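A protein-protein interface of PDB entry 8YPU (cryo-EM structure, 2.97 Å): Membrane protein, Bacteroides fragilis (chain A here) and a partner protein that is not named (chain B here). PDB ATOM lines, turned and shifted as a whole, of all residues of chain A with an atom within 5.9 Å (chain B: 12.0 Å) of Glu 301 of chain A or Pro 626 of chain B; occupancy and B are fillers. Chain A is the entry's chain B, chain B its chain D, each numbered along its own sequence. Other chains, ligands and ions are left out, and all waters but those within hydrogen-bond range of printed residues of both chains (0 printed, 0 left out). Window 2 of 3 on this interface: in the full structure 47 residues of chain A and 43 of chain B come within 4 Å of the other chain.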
ATOM      1  N   VAL A 186     -21.656 -28.730 -19.786  1.00  0.00           N
ATOM      2  CA  VAL A 186     -21.939 -27.889 -18.628  1.00  0.00           C
ATOM      3  C   VAL A 186     -21.669 -26.423 -18.937  1.00  0.00           C
ATOM      4  O   VAL A 186     -22.371 -25.537 -18.438  1.00  0.00           O
ATOM      5  CB  VAL A 186     -21.131 -28.372 -17.412  1.00  0.00           C
ATOM      6  CG1 VAL A 186     -21.761 -29.617 -16.833  1.00  0.00           C
ATOM      7  CG2 VAL A 186     -19.691 -28.642 -17.807  1.00  0.00           C
ATOM      8  N   ASN A 239     -35.422 -28.541 -26.725  1.00  0.00           N
ATOM      9  CA  ASN A 239     -35.108 -27.410 -25.865  1.00  0.00           C
ATOM     10  C   ASN A 239     -34.087 -27.768 -24.793  1.00  0.00           C
ATOM     11  O   ASN A 239     -33.461 -26.867 -24.228  1.00  0.00           O
ATOM     12  CB  ASN A 239     -36.397 -26.901 -25.221  1.00  0.00           C
ATOM     13  CG  ASN A 239     -36.319 -25.449 -24.819  1.00  0.00           C
ATOM     14  OD1 ASN A 239     -35.514 -24.688 -25.353  1.00  0.00           O
ATOM     15  ND2 ASN A 239     -37.170 -25.050 -23.883  1.00  0.00           N
ATOM     16  N   HIS A 240     -33.906 -29.054 -24.508  1.00  0.00           N
ATOM     17  CA  HIS A 240     -32.983 -29.487 -23.468  1.00  0.00           C
ATOM     18  C   HIS A 240     -31.544 -29.170 -23.854  1.00  0.00           C
ATOM     19  O   HIS A 240     -31.158 -29.272 -25.020  1.00  0.00           O
ATOM     20  CB  HIS A 240     -33.148 -30.985 -23.218  1.00  0.00           C
ATOM     21  CG  HIS A 240     -32.794 -31.414 -21.829  1.00  0.00           C
ATOM     22  ND1 HIS A 240     -31.511 -31.760 -21.461  1.00  0.00           N
ATOM     23  CD2 HIS A 240     -33.553 -31.556 -20.718  1.00  0.00           C
ATOM     24  CE1 HIS A 240     -31.496 -32.094 -20.184  1.00  0.00           C
ATOM     25  NE2 HIS A 240     -32.724 -31.981 -19.710  1.00  0.00           N
ATOM     26  N   PHE A 241     -30.744 -28.783 -22.857  1.00  0.00           N
ATOM     27  CA  PHE A 241     -29.361 -28.404 -23.125  1.00  0.00           C
ATOM     28  C   PHE A 241     -28.487 -29.612 -23.433  1.00  0.00           C
ATOM     29  O   PHE A 241     -27.450 -29.471 -24.090  1.00  0.00           O
ATOM     30  CB  PHE A 241     -28.796 -27.613 -21.946  1.00  0.00           C
ATOM     31  CG  PHE A 241     -28.317 -28.465 -20.807  1.00  0.00           C
ATOM     32  CD1 PHE A 241     -29.214 -29.010 -19.911  1.00  0.00           C
ATOM     33  CD2 PHE A 241     -26.968 -28.704 -20.623  1.00  0.00           C
ATOM     34  CE1 PHE A 241     -28.776 -29.784 -18.858  1.00  0.00           C
ATOM     35  CE2 PHE A 241     -26.528 -29.478 -19.574  1.00  0.00           C
ATOM     36  CZ  PHE A 241     -27.433 -30.017 -18.691  1.00  0.00           C
ATOM     37  N   GLU A 242     -28.878 -30.799 -22.967  1.00  0.00           N
ATOM     38  CA  GLU A 242     -28.141 -32.012 -23.288  1.00  0.00           C
ATOM     39  C   GLU A 242     -28.371 -32.474 -24.719  1.00  0.00           C
ATOM     40  O   GLU A 242     -27.655 -33.364 -25.187  1.00  0.00           O
ATOM     41  CB  GLU A 242     -28.530 -33.133 -22.325  1.00  0.00           C
ATOM     42  CG  GLU A 242     -27.971 -32.992 -20.924  1.00  0.00           C
ATOM     43  CD  GLU A 242     -26.554 -33.515 -20.804  1.00  0.00           C
ATOM     44  OE1 GLU A 242     -26.127 -34.286 -21.688  1.00  0.00           O
ATOM     45  OE2 GLU A 242     -25.872 -33.165 -19.819  1.00  0.00           O
ATOM     46  N   LYS A 299     -37.479 -24.612 -15.794  1.00  0.00           N
ATOM     47  CA  LYS A 299     -36.328 -25.029 -15.013  1.00  0.00           C
ATOM     48  C   LYS A 299     -35.073 -24.842 -15.851  1.00  0.00           C
ATOM     49  O   LYS A 299     -35.122 -24.855 -17.083  1.00  0.00           O
ATOM     50  CB  LYS A 299     -36.461 -26.481 -14.540  1.00  0.00           C
ATOM     51  CG  LYS A 299     -36.392 -27.520 -15.641  1.00  0.00           C
ATOM     52  CD  LYS A 299     -36.484 -28.925 -15.071  1.00  0.00           C
ATOM     53  CE  LYS A 299     -37.824 -29.183 -14.395  1.00  0.00           C
ATOM     54  NZ  LYS A 299     -38.947 -28.436 -15.027  1.00  0.00           N
ATOM     55  N   ARG A 300     -33.946 -24.668 -15.164  1.00  0.00           N
ATOM     56  CA  ARG A 300     -32.727 -24.205 -15.816  1.00  0.00           C
ATOM     57  C   ARG A 300     -32.173 -25.202 -16.827  1.00  0.00           C
ATOM     58  O   ARG A 300     -31.334 -24.825 -17.650  1.00  0.00           O
ATOM     59  CB  ARG A 300     -31.670 -23.883 -14.763  1.00  0.00           C
ATOM     60  CG  ARG A 300     -30.613 -22.915 -15.237  1.00  0.00           C
ATOM     61  CD  ARG A 300     -31.160 -21.505 -15.372  1.00  0.00           C
ATOM     62  NE  ARG A 300     -30.487 -20.751 -16.423  1.00  0.00           N
ATOM     63  CZ  ARG A 300     -29.811 -19.628 -16.226  1.00  0.00           C
ATOM     64  NH1 ARG A 300     -29.683 -19.101 -15.020  1.00  0.00           N
ATOM     65  NH2 ARG A 300     -29.248 -19.019 -17.264  1.00  0.00           N
ATOM     66  N   GLU A 301     -32.615 -26.460 -16.788  1.00  0.00           N
ATOM     67  CA  GLU A 301     -32.112 -27.447 -17.736  1.00  0.00           C
ATOM     68  C   GLU A 301     -32.700 -27.273 -19.130  1.00  0.00           C
ATOM     69  O   GLU A 301     -32.148 -27.816 -20.090  1.00  0.00           O
ATOM     70  CB  GLU A 301     -32.385 -28.858 -17.216  1.00  0.00           C
ATOM     71  CG  GLU A 301     -33.672 -29.470 -17.716  1.00  0.00           C
ATOM     72  CD  GLU A 301     -34.120 -30.635 -16.864  1.00  0.00           C
ATOM     73  OE1 GLU A 301     -33.762 -30.665 -15.669  1.00  0.00           O
ATOM     74  OE2 GLU A 301     -34.830 -31.519 -17.387  1.00  0.00           O
ATOM     75  N   PHE A 302     -33.804 -26.539 -19.263  1.00  0.00           N
ATOM     76  CA  PHE A 302     -34.369 -26.230 -20.575  1.00  0.00           C
ATOM     77  C   PHE A 302     -33.917 -24.836 -21.004  1.00  0.00           C
ATOM     78  O   PHE A 302     -34.708 -23.921 -21.225  1.00  0.00           O
ATOM     79  CB  PHE A 302     -35.889 -26.344 -20.539  1.00  0.00           C
ATOM     80  CG  PHE A 302     -36.382 -27.730 -20.255  1.00  0.00           C
ATOM     81  CD1 PHE A 302     -36.217 -28.741 -21.181  1.00  0.00           C
ATOM     82  CD2 PHE A 302     -36.999 -28.024 -19.054  1.00  0.00           C
ATOM     83  CE1 PHE A 302     -36.659 -30.014 -20.915  1.00  0.00           C
ATOM     84  CE2 PHE A 302     -37.446 -29.295 -18.787  1.00  0.00           C
ATOM     85  CZ  PHE A 302     -37.276 -30.292 -19.718  1.00  0.00           C
ATOM     86  N   SER A 303     -32.600 -24.699 -21.126  1.00  0.00           N
ATOM     87  CA  SER A 303     -31.963 -23.453 -21.521  1.00  0.00           C
ATOM     88  C   SER A 303     -31.527 -23.570 -22.970  1.00  0.00           C
ATOM     89  O   SER A 303     -30.836 -24.524 -23.336  1.00  0.00           O
ATOM     90  CB  SER A 303     -30.754 -23.142 -20.637  1.00  0.00           C
ATOM     91  OG  SER A 303     -31.094 -23.177 -19.265  1.00  0.00           O
ATOM     92  N   VAL B 621     -19.485 -18.728  -6.128  1.00  0.00           N
ATOM     93  CA  VAL B 621     -19.590 -19.992  -6.848  1.00  0.00           C
ATOM     94  C   VAL B 621     -21.046 -20.255  -7.203  1.00  0.00           C
ATOM     95  O   VAL B 621     -21.796 -20.834  -6.411  1.00  0.00           O
ATOM     96  CB  VAL B 621     -19.005 -21.156  -6.030  1.00  0.00           C
ATOM     97  CG1 VAL B 621     -18.701 -22.328  -6.938  1.00  0.00           C
ATOM     98  CG2 VAL B 621     -17.753 -20.711  -5.302  1.00  0.00           C
ATOM     99  N   ASP B 622     -21.458 -19.817  -8.386  1.00  0.00           N
ATOM    100  CA  ASP B 622     -22.795 -20.082  -8.891  1.00  0.00           C
ATOM    101  C   ASP B 622     -22.697 -20.957 -10.137  1.00  0.00           C
ATOM    102  O   ASP B 622     -21.611 -21.370 -10.548  1.00  0.00           O
ATOM    103  CB  ASP B 622     -23.526 -18.771  -9.165  1.00  0.00           C
ATOM    104  CG  ASP B 622     -25.005 -18.856  -8.874  1.00  0.00           C
ATOM    105  OD1 ASP B 622     -25.605 -19.914  -9.146  1.00  0.00           O
ATOM    106  OD2 ASP B 622     -25.570 -17.861  -8.378  1.00  0.00           O
ATOM    107  N   ASN B 623     -23.837 -21.242 -10.759  1.00  0.00           N
ATOM    108  CA  ASN B 623     -23.866 -22.117 -11.921  1.00  0.00           C
ATOM    109  C   ASN B 623     -24.998 -21.682 -12.842  1.00  0.00           C
ATOM    110  O   ASN B 623     -26.071 -21.296 -12.376  1.00  0.00           O
ATOM    111  CB  ASN B 623     -24.020 -23.584 -11.496  1.00  0.00           C
ATOM    112  CG  ASN B 623     -25.461 -23.992 -11.283  1.00  0.00           C
ATOM    113  OD1 ASN B 623     -26.180 -23.388 -10.489  1.00  0.00           O
ATOM    114  ND2 ASN B 623     -25.889 -25.030 -11.987  1.00  0.00           N
ATOM    115  N   ILE B 624     -24.743 -21.733 -14.149  1.00  0.00           N
ATOM    116  CA  ILE B 624     -25.730 -21.311 -15.136  1.00  0.00           C
ATOM    117  C   ILE B 624     -26.470 -22.531 -15.663  1.00  0.00           C
ATOM    118  O   ILE B 624     -27.691 -22.501 -15.836  1.00  0.00           O
ATOM    119  CB  ILE B 624     -25.082 -20.518 -16.285  1.00  0.00           C
ATOM    120  CG1 ILE B 624     -24.592 -19.165 -15.786  1.00  0.00           C
ATOM    121  CG2 ILE B 624     -26.064 -20.310 -17.416  1.00  0.00           C
ATOM    122  CD1 ILE B 624     -23.423 -18.621 -16.535  1.00  0.00           C
ATOM    123  N   LEU B 625     -25.742 -23.613 -15.920  1.00  0.00           N
ATOM    124  CA  LEU B 625     -26.331 -24.848 -16.405  1.00  0.00           C
ATOM    125  C   LEU B 625     -26.249 -25.906 -15.316  1.00  0.00           C
ATOM    126  O   LEU B 625     -25.321 -25.869 -14.497  1.00  0.00           O
ATOM    127  CB  LEU B 625     -25.612 -25.337 -17.665  1.00  0.00           C
ATOM    128  CG  LEU B 625     -26.127 -24.769 -18.985  1.00  0.00           C
ATOM    129  CD1 LEU B 625     -25.490 -25.488 -20.148  1.00  0.00           C
ATOM    130  CD2 LEU B 625     -27.635 -24.869 -19.059  1.00  0.00           C
ATOM    131  N   PRO B 626     -27.197 -26.839 -15.248  1.00  0.00           N
ATOM    132  CA  PRO B 626     -27.124 -27.889 -14.226  1.00  0.00           C
ATOM    133  C   PRO B 626     -25.865 -28.725 -14.373  1.00  0.00           C
ATOM    134  O   PRO B 626     -25.467 -29.097 -15.479  1.00  0.00           O
ATOM    135  CB  PRO B 626     -28.384 -28.719 -14.489  1.00  0.00           C
ATOM    136  CG  PRO B 626     -29.314 -27.788 -15.163  1.00  0.00           C
ATOM    137  CD  PRO B 626     -28.454 -26.902 -16.011  1.00  0.00           C
ATOM    138  N   GLY B 627     -25.240 -29.033 -13.242  1.00  0.00           N
ATOM    139  CA  GLY B 627     -24.061 -29.863 -13.226  1.00  0.00           C
ATOM    140  C   GLY B 627     -22.756 -29.135 -13.452  1.00  0.00           C
ATOM    141  O   GLY B 627     -21.691 -29.728 -13.243  1.00  0.00           O
ATOM    142  N   GLY B 628     -22.795 -27.876 -13.871  1.00  0.00           N
ATOM    143  CA  GLY B 628     -21.563 -27.150 -14.085  1.00  0.00           C
ATOM    144  C   GLY B 628     -21.452 -25.921 -13.214  1.00  0.00           C
ATOM    145  O   GLY B 628     -22.131 -24.921 -13.446  1.00  0.00           O
ATOM    146  N   SER B 629     -20.565 -25.981 -12.227  1.00  0.00           N
ATOM    147  CA  SER B 629     -20.379 -24.922 -11.249  1.00  0.00           C
ATOM    148  C   SER B 629     -18.992 -24.334 -11.437  1.00  0.00           C
ATOM    149  O   SER B 629     -18.030 -25.069 -11.674  1.00  0.00           O
ATOM    150  CB  SER B 629     -20.547 -25.454  -9.825  1.00  0.00           C
ATOM    151  OG  SER B 629     -20.608 -24.399  -8.886  1.00  0.00           O
ATOM    152  N   GLU B 630     -18.894 -23.011 -11.341  1.00  0.00           N
ATOM    153  CA  GLU B 630     -17.637 -22.321 -11.565  1.00  0.00           C
ATOM    154  C   GLU B 630     -17.621 -21.042 -10.750  1.00  0.00           C
ATOM    155  O   GLU B 630     -18.659 -20.557 -10.297  1.00  0.00           O
ATOM    156  CB  GLU B 630     -17.427 -22.010 -13.045  1.00  0.00           C
ATOM    157  CG  GLU B 630     -18.484 -21.100 -13.607  1.00  0.00           C
ATOM    158  CD  GLU B 630     -18.239 -20.754 -15.052  1.00  0.00           C
ATOM    159  OE1 GLU B 630     -17.120 -21.000 -15.548  1.00  0.00           O
ATOM    160  OE2 GLU B 630     -19.164 -20.220 -15.688  1.00  0.00           O
ATOM    161  N   MET B 632     -17.426 -17.146 -10.173  1.00  0.00           N
ATOM    162  CA  MET B 632     -17.880 -15.955 -10.868  1.00  0.00           C
ATOM    163  C   MET B 632     -17.563 -14.740 -10.013  1.00  0.00           C
ATOM    164  O   MET B 632     -17.501 -14.831  -8.786  1.00  0.00           O
ATOM    165  CB  MET B 632     -19.380 -16.008 -11.159  1.00  0.00           C
ATOM    166  CG  MET B 632     -19.882 -17.367 -11.587  1.00  0.00           C
ATOM    167  SD  MET B 632     -21.668 -17.411 -11.737  1.00  0.00           S
ATOM    168  CE  MET B 632     -21.840 -18.158 -13.345  1.00  0.00           C
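His 240 of chain A touches none of the printed residues of chain B.
Phe 241 of chain A touches just these residues of chain B: Leu 625 and Pro 626.
Of the printed residues of chain B, Arg 300 of chain A touches Ile 624 (3.0 Å), Leu 625 (3.96 Å) and Pro 626 (3.9 Å).
Of the printed residues of chain B, Glu 301 of chain A touches Pro 626 (3.8 Å).
Ser 303 of chain A touches one residue of chain B.
Asp 622 of chain B touches none of the printed residues of chain A.
Of the printed residues of chain A, Ile 624 of chain B touches Arg 300 (3.0 Å).
Printed residues of chain A within 4 Å of Leu 625 of chain B: Val 186 (3.3 Å), Phe 241 (3.6 Å), Arg 300 (3.96 Å) and Ser 303 (3.9 Å).
Of chain A, only Val 186, Phe 241, Arg 300 and Glu 301 come within 4 Å of Pro 626 of chain B.
Printed residues of chain A within 4 Å of Gly 627 of chain B: Val 186 (3.6 Å).
Printed residues of chain A within 4 Å of Gly 628 of chain B: Val 186.
Met 632 of chain B touches none of the printed residues of chain A.
The nearest residue of chain B that does not touch Glu 301 of chain A is Leu 625 of chain B (5.3 Å).
The nearest printed residue of chain A that does not touch Ile 624 of chain B is Ser 303 of chain A (4.9 Å).
Leu 625 of chain B touches Val 186 of chain A.
O of Pro 626 of chain B touches CG1 of Val 186 of chain A, 3.98 Å away.
Gly 627 of chain B touches Val 186 of chain A (C to CG1, 3.6 Å).
Gly 628 of chain B touches Val 186 of chain A.
Phe 241 of chain A touches Leu 625 of chain B.
Phe 241 of chain A touches Pro 626 of chain B.
O of Arg 300 of chain A touches CD2 of Leu 625 of chain B, at 3.96 Å.
Pro 626 of chain B touches Arg 300 of chain A (CD to O, 3.9 Å).
CA of Glu 301 of chain A touches CG of Pro 626 of chain B, at 3.8 Å.
Leu 625 of chain B touches Ser 303 of chain A (CD2 to OG, 3.9 Å).
Hydrophobic or aromatic side chains of chain A within 4 Å of the printed part of chain B: Val 186 and Phe 241.
Of the 11 printed residues of chain B, 5 touch a printed residue of chain A.
Hydrophobic or aromatic side chains of chain B that line the printed part of chain A: Ile 624, Leu 625 and Pro 626.
Among the printed residues, 11 pairs touch across the chains.
The backbone carbonyl oxygen (O) of Ile 624 of chain B lies close to the guanidinium group (NE) of Arg 300 of chain A, at 3.4 Å.
The side-chain amide nitrogen of Asn 623 of chain B lies within hydrogen-bond range of the backbone carbonyl oxygen of Leu 625 of chain B (2.7 Å).
OE2 of Glu 301 of chain A lies within hydrogen-bond range of NE2 of His 240 of chain A.
The backbone NH of Phe 241 of chain A lies close to the backbone carbonyl oxygen of Glu 301 of chain A (3.3 Å).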
